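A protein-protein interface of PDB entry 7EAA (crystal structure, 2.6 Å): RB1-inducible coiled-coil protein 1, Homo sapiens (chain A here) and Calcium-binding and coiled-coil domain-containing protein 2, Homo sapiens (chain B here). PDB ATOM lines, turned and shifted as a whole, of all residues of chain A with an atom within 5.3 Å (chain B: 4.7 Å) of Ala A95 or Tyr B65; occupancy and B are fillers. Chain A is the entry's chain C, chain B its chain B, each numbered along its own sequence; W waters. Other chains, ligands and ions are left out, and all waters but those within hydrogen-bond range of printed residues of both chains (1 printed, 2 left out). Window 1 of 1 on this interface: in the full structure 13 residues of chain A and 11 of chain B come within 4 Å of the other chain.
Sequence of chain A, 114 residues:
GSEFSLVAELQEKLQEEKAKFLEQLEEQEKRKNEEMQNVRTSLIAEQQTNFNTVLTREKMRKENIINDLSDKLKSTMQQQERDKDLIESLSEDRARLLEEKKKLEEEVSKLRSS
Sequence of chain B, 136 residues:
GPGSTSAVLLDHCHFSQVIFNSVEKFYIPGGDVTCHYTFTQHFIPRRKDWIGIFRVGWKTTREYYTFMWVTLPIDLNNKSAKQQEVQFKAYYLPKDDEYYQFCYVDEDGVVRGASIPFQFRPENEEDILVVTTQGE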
ATOM      1  N   GLU A  88     -19.973 -10.141   5.625  1.00  0.00           N
ATOM      2  CA  GLU A  88     -20.574  -9.959   6.950  1.00  0.00           C
ATOM      3  C   GLU A  88     -20.044  -8.701   7.622  1.00  0.00           C
ATOM      4  O   GLU A  88     -20.815  -7.885   8.135  1.00  0.00           O
ATOM      5  CB  GLU A  88     -20.294 -11.163   7.841  1.00  0.00           C
ATOM      6  CG  GLU A  88     -21.239 -12.322   7.726  1.00  0.00           C
ATOM      7  CD  GLU A  88     -20.656 -13.564   8.374  1.00  0.00           C
ATOM      8  OE1 GLU A  88     -19.638 -13.434   9.094  1.00  0.00           O
ATOM      9  OE2 GLU A  88     -21.203 -14.668   8.163  1.00  0.00           O
ATOM     10  N   LEU A  90     -18.577  -6.057   6.143  1.00  0.00           N
ATOM     11  CA  LEU A  90     -18.893  -4.841   5.392  1.00  0.00           C
ATOM     12  C   LEU A  90     -20.366  -4.491   5.499  1.00  0.00           C
ATOM     13  O   LEU A  90     -20.720  -3.349   5.785  1.00  0.00           O
ATOM     14  CB  LEU A  90     -18.511  -4.990   3.921  1.00  0.00           C
ATOM     15  CG  LEU A  90     -17.032  -4.973   3.569  1.00  0.00           C
ATOM     16  CD1 LEU A  90     -16.850  -5.043   2.072  1.00  0.00           C
ATOM     17  CD2 LEU A  90     -16.362  -3.740   4.129  1.00  0.00           C
ATOM     18  N   SER A  91     -21.249  -5.451   5.265  1.00  0.00           N
ATOM     19  CA  SER A  91     -22.661  -5.106   5.279  1.00  0.00           C
ATOM     20  C   SER A  91     -23.077  -4.571   6.648  1.00  0.00           C
ATOM     21  O   SER A  91     -23.875  -3.633   6.734  1.00  0.00           O
ATOM     22  CB  SER A  91     -23.507  -6.313   4.869  1.00  0.00           C
ATOM     23  OG  SER A  91     -23.304  -7.415   5.723  1.00  0.00           O
ATOM     24  N   GLU A  92     -22.503  -5.122   7.728  1.00  0.00           N
ATOM     25  CA  GLU A  92     -22.861  -4.684   9.077  1.00  0.00           C
ATOM     26  C   GLU A  92     -22.297  -3.302   9.375  1.00  0.00           C
ATOM     27  O   GLU A  92     -22.993  -2.445   9.924  1.00  0.00           O
ATOM     28  CB  GLU A  92     -22.356  -5.686  10.115  1.00  0.00           C
ATOM     29  CG  GLU A  92     -23.189  -5.742  11.381  1.00  0.00           C
ATOM     30  CD  GLU A  92     -22.900  -4.587  12.361  1.00  0.00           C
ATOM     31  OE1 GLU A  92     -23.859  -4.111  13.026  1.00  0.00           O
ATOM     32  OE2 GLU A  92     -21.726  -4.157  12.475  1.00  0.00           O
ATOM     33  N   ASP A  93     -21.029  -3.065   9.046  1.00  0.00           N
ATOM     34  CA  ASP A  93     -20.478  -1.758   9.347  1.00  0.00           C
ATOM     35  C   ASP A  93     -21.155  -0.673   8.522  1.00  0.00           C
ATOM     36  O   ASP A  93     -21.363   0.449   9.004  1.00  0.00           O
ATOM     37  CB  ASP A  93     -18.975  -1.724   9.130  1.00  0.00           C
ATOM     38  CG  ASP A  93     -18.379  -0.406   9.616  1.00  0.00           C
ATOM     39  OD1 ASP A  93     -18.604  -0.082  10.811  1.00  0.00           O
ATOM     40  OD2 ASP A  93     -17.736   0.317   8.811  1.00  0.00           O
ATOM     41  N   ARG A  94     -21.504  -0.984   7.279  1.00  0.00           N
ATOM     42  CA  ARG A  94     -22.144   0.008   6.435  1.00  0.00           C
ATOM     43  C   ARG A  94     -23.501   0.398   6.989  1.00  0.00           C
ATOM     44  O   ARG A  94     -23.867   1.576   6.966  1.00  0.00           O
ATOM     45  CB  ARG A  94     -22.260  -0.518   5.012  1.00  0.00           C
ATOM     46  CG  ARG A  94     -22.387   0.555   3.988  1.00  0.00           C
ATOM     47  CD  ARG A  94     -22.546  -0.042   2.620  1.00  0.00           C
ATOM     48  NE  ARG A  94     -23.543   0.672   1.843  1.00  0.00           N
ATOM     49  CZ  ARG A  94     -24.760   0.210   1.591  1.00  0.00           C
ATOM     50  NH1 ARG A  94     -25.134  -0.970   2.052  1.00  0.00           N
ATOM     51  NH2 ARG A  94     -25.593   0.933   0.865  1.00  0.00           N
ATOM     52  N   ALA A  95     -24.256  -0.570   7.509  1.00  0.00           N
ATOM     53  CA  ALA A  95     -25.566  -0.246   8.072  1.00  0.00           C
ATOM     54  C   ALA A  95     -25.439   0.658   9.308  1.00  0.00           C
ATOM     55  O   ALA A  95     -26.330   1.467   9.583  1.00  0.00           O
ATOM     56  CB  ALA A  95     -26.324  -1.528   8.401  1.00  0.00           C
ATOM     57  N   ARG A  96     -24.338   0.557  10.054  1.00  0.00           N
ATOM     58  CA  ARG A  96     -24.165   1.425  11.205  1.00  0.00           C
ATOM     59  C   ARG A  96     -23.789   2.823  10.758  1.00  0.00           C
ATOM     60  O   ARG A  96     -24.378   3.809  11.216  1.00  0.00           O
ATOM     61  CB  ARG A  96     -23.124   0.841  12.155  1.00  0.00           C
ATOM     62  CG  ARG A  96     -23.549  -0.538  12.704  1.00  0.00           C
ATOM     63  CD  ARG A  96     -24.699  -0.460  13.731  1.00  0.00           C
ATOM     64  NE  ARG A  96     -26.019  -0.096  13.190  1.00  0.00           N
ATOM     65  CZ  ARG A  96     -26.879  -0.949  12.628  1.00  0.00           C
ATOM     66  NH1 ARG A  96     -26.568  -2.236  12.514  1.00  0.00           N
ATOM     67  NH2 ARG A  96     -28.056  -0.515  12.181  1.00  0.00           N
ATOM     68  N   LEU A  97     -22.830   2.919   9.835  1.00  0.00           N
ATOM     69  CA  LEU A  97     -22.488   4.192   9.209  1.00  0.00           C
ATOM     70  C   LEU A  97     -23.729   4.909   8.692  1.00  0.00           C
ATOM     71  O   LEU A  97     -23.890   6.117   8.901  1.00  0.00           O
ATOM     72  CB  LEU A  97     -21.503   3.957   8.071  1.00  0.00           C
ATOM     73  CG  LEU A  97     -20.061   3.755   8.506  1.00  0.00           C
ATOM     74  CD1 LEU A  97     -19.216   3.137   7.397  1.00  0.00           C
ATOM     75  CD2 LEU A  97     -19.490   5.091   8.945  1.00  0.00           C
ATOM     76  N   LEU A  98     -24.622   4.179   8.007  1.00  0.00           N
ATOM     77  CA  LEU A  98     -25.866   4.784   7.541  1.00  0.00           C
ATOM     78  C   LEU A  98     -26.643   5.386   8.696  1.00  0.00           C
ATOM     79  O   LEU A  98     -27.159   6.504   8.590  1.00  0.00           O
ATOM     80  CB  LEU A  98     -26.722   3.759   6.798  1.00  0.00           C
ATOM     81  CG  LEU A  98     -26.353   3.626   5.319  1.00  0.00           C
ATOM     82  CD1 LEU A  98     -27.075   2.462   4.618  1.00  0.00           C
ATOM     83  CD2 LEU A  98     -26.596   4.952   4.607  1.00  0.00           C
ATOM     84  N   GLU A  99     -26.724   4.668   9.818  1.00  0.00           N
ATOM     85  CA  GLU A  99     -27.438   5.189  10.980  1.00  0.00           C
ATOM     86  C   GLU A  99     -26.690   6.359  11.607  1.00  0.00           C
ATOM     87  O   GLU A  99     -27.299   7.364  11.999  1.00  0.00           O
ATOM     88  CB  GLU A  99     -27.649   4.074  12.003  1.00  0.00           C
ATOM     89  CG  GLU A  99     -28.733   3.079  11.628  1.00  0.00           C
ATOM     90  CD  GLU A  99     -30.089   3.748  11.351  1.00  0.00           C
ATOM     91  OE1 GLU A  99     -30.672   3.490  10.269  1.00  0.00           O
ATOM     92  OE2 GLU A  99     -30.575   4.523  12.217  1.00  0.00           O
ATOM     93  N   ILE B  53     -32.314  -5.952   0.044  1.00  0.00           N
ATOM     94  CA  ILE B  53     -32.918  -6.044   1.369  1.00  0.00           C
ATOM     95  C   ILE B  53     -32.833  -4.669   1.992  1.00  0.00           C
ATOM     96  O   ILE B  53     -31.734  -4.135   2.162  1.00  0.00           O
ATOM     97  CB  ILE B  53     -32.192  -7.075   2.247  1.00  0.00           C
ATOM     98  CG1 ILE B  53     -32.325  -8.462   1.640  1.00  0.00           C
ATOM     99  CG2 ILE B  53     -32.683  -7.020   3.687  1.00  0.00           C
ATOM    100  CD1 ILE B  53     -31.504  -9.474   2.360  1.00  0.00           C
ATOM    101  N   GLU B  63     -29.764   2.803   0.366  1.00  0.00           N
ATOM    102  CA  GLU B  63     -29.802   2.320   1.735  1.00  0.00           C
ATOM    103  C   GLU B  63     -29.986   0.806   1.846  1.00  0.00           C
ATOM    104  O   GLU B  63     -30.340   0.317   2.927  1.00  0.00           O
ATOM    105  CB  GLU B  63     -30.907   3.045   2.496  1.00  0.00           C
ATOM    106  CG  GLU B  63     -30.464   4.392   3.029  1.00  0.00           C
ATOM    107  CD  GLU B  63     -31.620   5.253   3.525  1.00  0.00           C
ATOM    108  OE1 GLU B  63     -31.681   6.452   3.154  1.00  0.00           O
ATOM    109  OE2 GLU B  63     -32.460   4.733   4.287  1.00  0.00           O
ATOM    110  N   TYR B  64     -29.760   0.055   0.768  1.00  0.00           N
ATOM    111  CA  TYR B  64     -29.920  -1.389   0.845  1.00  0.00           C
ATOM    112  C   TYR B  64     -28.931  -1.956   1.865  1.00  0.00           C
ATOM    113  O   TYR B  64     -27.834  -1.426   2.056  1.00  0.00           O
ATOM    114  CB  TYR B  64     -29.700  -2.023  -0.540  1.00  0.00           C
ATOM    115  CG  TYR B  64     -28.295  -1.824  -1.042  1.00  0.00           C
ATOM    116  CD1 TYR B  64     -27.979  -0.767  -1.890  1.00  0.00           C
ATOM    117  CD2 TYR B  64     -27.259  -2.675  -0.632  1.00  0.00           C
ATOM    118  CE1 TYR B  64     -26.666  -0.568  -2.322  1.00  0.00           C
ATOM    119  CE2 TYR B  64     -25.964  -2.480  -1.041  1.00  0.00           C
ATOM    120  CZ  TYR B  64     -25.671  -1.427  -1.895  1.00  0.00           C
ATOM    121  OH  TYR B  64     -24.373  -1.241  -2.303  1.00  0.00           O
ATOM    122  N   TYR B  65     -29.331  -3.041   2.525  1.00  0.00           N
ATOM    123  CA  TYR B  65     -28.393  -3.818   3.330  1.00  0.00           C
ATOM    124  C   TYR B  65     -27.463  -4.652   2.439  1.00  0.00           C
ATOM    125  O   TYR B  65     -26.242  -4.513   2.505  1.00  0.00           O
ATOM    126  CB  TYR B  65     -29.158  -4.709   4.314  1.00  0.00           C
ATOM    127  CG  TYR B  65     -28.242  -5.354   5.297  1.00  0.00           C
ATOM    128  CD1 TYR B  65     -27.857  -6.678   5.157  1.00  0.00           C
ATOM    129  CD2 TYR B  65     -27.713  -4.628   6.360  1.00  0.00           C
ATOM    130  CE1 TYR B  65     -26.977  -7.271   6.069  1.00  0.00           C
ATOM    131  CE2 TYR B  65     -26.847  -5.219   7.281  1.00  0.00           C
ATOM    132  CZ  TYR B  65     -26.480  -6.537   7.112  1.00  0.00           C
ATOM    133  OH  TYR B  65     -25.618  -7.109   7.998  1.00  0.00           O
ATOM    134  N   THR B  66     -28.026  -5.526   1.601  1.00  0.00           N
ATOM    135  CA  THR B  66     -27.311  -6.173   0.505  1.00  0.00           C
ATOM    136  C   THR B  66     -28.264  -6.221  -0.674  1.00  0.00           C
ATOM    137  O   THR B  66     -29.447  -5.867  -0.557  1.00  0.00           O
ATOM    138  CB  THR B  66     -26.834  -7.603   0.842  1.00  0.00           C
ATOM    139  OG1 THR B  66     -27.919  -8.360   1.415  1.00  0.00           O
ATOM    140  CG2 THR B  66     -25.631  -7.608   1.801  1.00  0.00           C
ATOM    141  N   TYR B  92     -25.407 -12.781   3.448  1.00  0.00           N
ATOM    142  CA  TYR B  92     -26.002 -11.563   2.914  1.00  0.00           C
ATOM    143  C   TYR B  92     -27.025 -10.947   3.861  1.00  0.00           C
ATOM    144  O   TYR B  92     -27.553  -9.868   3.559  1.00  0.00           O
ATOM    145  CB  TYR B  92     -26.718 -11.852   1.582  1.00  0.00           C
ATOM    146  CG  TYR B  92     -25.842 -11.956   0.359  1.00  0.00           C
ATOM    147  CD1 TYR B  92     -26.192 -11.315  -0.831  1.00  0.00           C
ATOM    148  CD2 TYR B  92     -24.661 -12.718   0.378  1.00  0.00           C
ATOM    149  CE1 TYR B  92     -25.362 -11.420  -1.972  1.00  0.00           C
ATOM    150  CE2 TYR B  92     -23.848 -12.816  -0.741  1.00  0.00           C
ATOM    151  CZ  TYR B  92     -24.201 -12.172  -1.903  1.00  0.00           C
ATOM    152  OH  TYR B  92     -23.377 -12.279  -2.996  1.00  0.00           O
ATOM    153  N   LEU B  93     -27.368 -11.648   5.031  1.00  0.00           N
ATOM    154  CA  LEU B  93     -28.578 -11.244   5.737  1.00  0.00           C
ATOM    155  C   LEU B  93     -28.246 -10.449   6.980  1.00  0.00           C
ATOM    156  O   LEU B  93     -27.204 -10.659   7.599  1.00  0.00           O
ATOM    157  CB  LEU B  93     -29.415 -12.450   6.163  1.00  0.00           C
ATOM    158  CG  LEU B  93     -29.796 -13.361   5.017  1.00  0.00           C
ATOM    159  CD1 LEU B  93     -30.553 -14.560   5.551  1.00  0.00           C
ATOM    160  CD2 LEU B  93     -30.622 -12.580   3.988  1.00  0.00           C
ATOM    161  N   PRO B  94     -29.139  -9.549   7.367  1.00  0.00           N
ATOM    162  CA  PRO B  94     -28.959  -8.835   8.636  1.00  0.00           C
ATOM    163  C   PRO B  94     -28.986  -9.791   9.819  1.00  0.00           C
ATOM    164  O   PRO B  94     -29.552 -10.880   9.750  1.00  0.00           O
ATOM    165  CB  PRO B  94     -30.147  -7.870   8.669  1.00  0.00           C
ATOM    166  CG  PRO B  94     -30.507  -7.675   7.223  1.00  0.00           C
ATOM    167  CD  PRO B  94     -30.259  -9.014   6.578  1.00  0.00           C
ATOM    168  N   LYS B  95     -28.345  -9.374  10.909  1.00  0.00           N
ATOM    169  CA  LYS B  95     -28.309 -10.152  12.140  1.00  0.00           C
ATOM    170  C   LYS B  95     -29.147  -9.555  13.266  1.00  0.00           C
ATOM    171  O   LYS B  95     -29.266 -10.181  14.324  1.00  0.00           O
ATOM    172  CB  LYS B  95     -26.861 -10.313  12.618  1.00  0.00           C
ATOM    173  CG  LYS B  95     -25.928 -10.899  11.564  1.00  0.00           C
ATOM    174  CD  LYS B  95     -26.537 -12.133  10.915  1.00  0.00           C
ATOM    175  CE  LYS B  95     -25.753 -12.572   9.685  1.00  0.00           C
ATOM    176  NZ  LYS B  95     -24.292 -12.732   9.956  1.00  0.00           N
HETATM  177  O   HOH W   1     -24.997  -2.624   4.377  1.00  0.00           O
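OG of Ser A91 is in hydrogen-bond range of OH of Tyr B65.
The guanidinium group (NH1) of Arg A94 sits at hydrogen-bond distance from the backbone carbonyl oxygen (O) of Tyr B64 (2.7 Å).
The backbone carbonyl oxygen of Glu A88 sits at hydrogen-bond distance from the side-chain hydroxyl of Ser A91.
NH1 of Arg A96 lies within salt-bridge range of OE1 of Glu A92 (3.3 Å).
The backbone carbonyl oxygen (O) of Ile B53 sits at hydrogen-bond distance from the backbone NH (N) of Tyr B65, 2.7 Å away.
N of Ile B53 sits at hydrogen-bond distance from O of Thr B66 (2.9 Å).
The backbone carbonyl oxygen of Tyr B92 sits at hydrogen-bond distance from the side-chain hydroxyl of Thr B66.
CG of Glu A88 touches NZ of Lys B95, 3.8 Å away.
CB of Ser A91 touches CG2 of Thr B66, at 3.9 Å.
Tyr B65 touches Glu A92 (OH to N, 3.7 Å).
Arg A94 touches Tyr B65 (NH1 to O, 3.7 Å).
Ala A95 touches Tyr B65.
CA of Glu B63 touches CD1 of Leu A98 (3.97 Å).
Ala A95 touches just one residue of chain B: Tyr B65.
Tyr B65 touches just these residues of chain A: Ser A91, Glu A92, Arg A94 and Ala A95.
Printed residues of chain A within 4 Å of Thr B66: Ser A91.
Of the printed residues of chain B, Glu A88 touches Lys B95.
Printed residues of chain A within 4 Å of Lys B95: Glu A88 (3.8 Å).
The nearest residue of chain A that does not touch Tyr B65 is Glu A88 (4.9 Å).
The nearest printed residue of chain A that does not touch Thr B66 is Arg A94 (5.4 Å).
Hydrophobic or aromatic side chains of chain A within 4 Å of the printed part of chain B: Ala A95 and Leu A98.
Of the 9 printed residues of chain B, 5 touch a printed residue of chain A.
Printed residues of chain B that touch a printed residue of chain A: Glu B63, Tyr B64, Tyr B65, Thr B66 and Lys B95.
Among the printed residues, 8 pairs touch across the chains.
Water W1 lies within hydrogen-bond range of O of Ser A91 (2.8 Å), NH1 of Arg A94 (2.9 Å) and O of Tyr B65 (2.9 Å).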
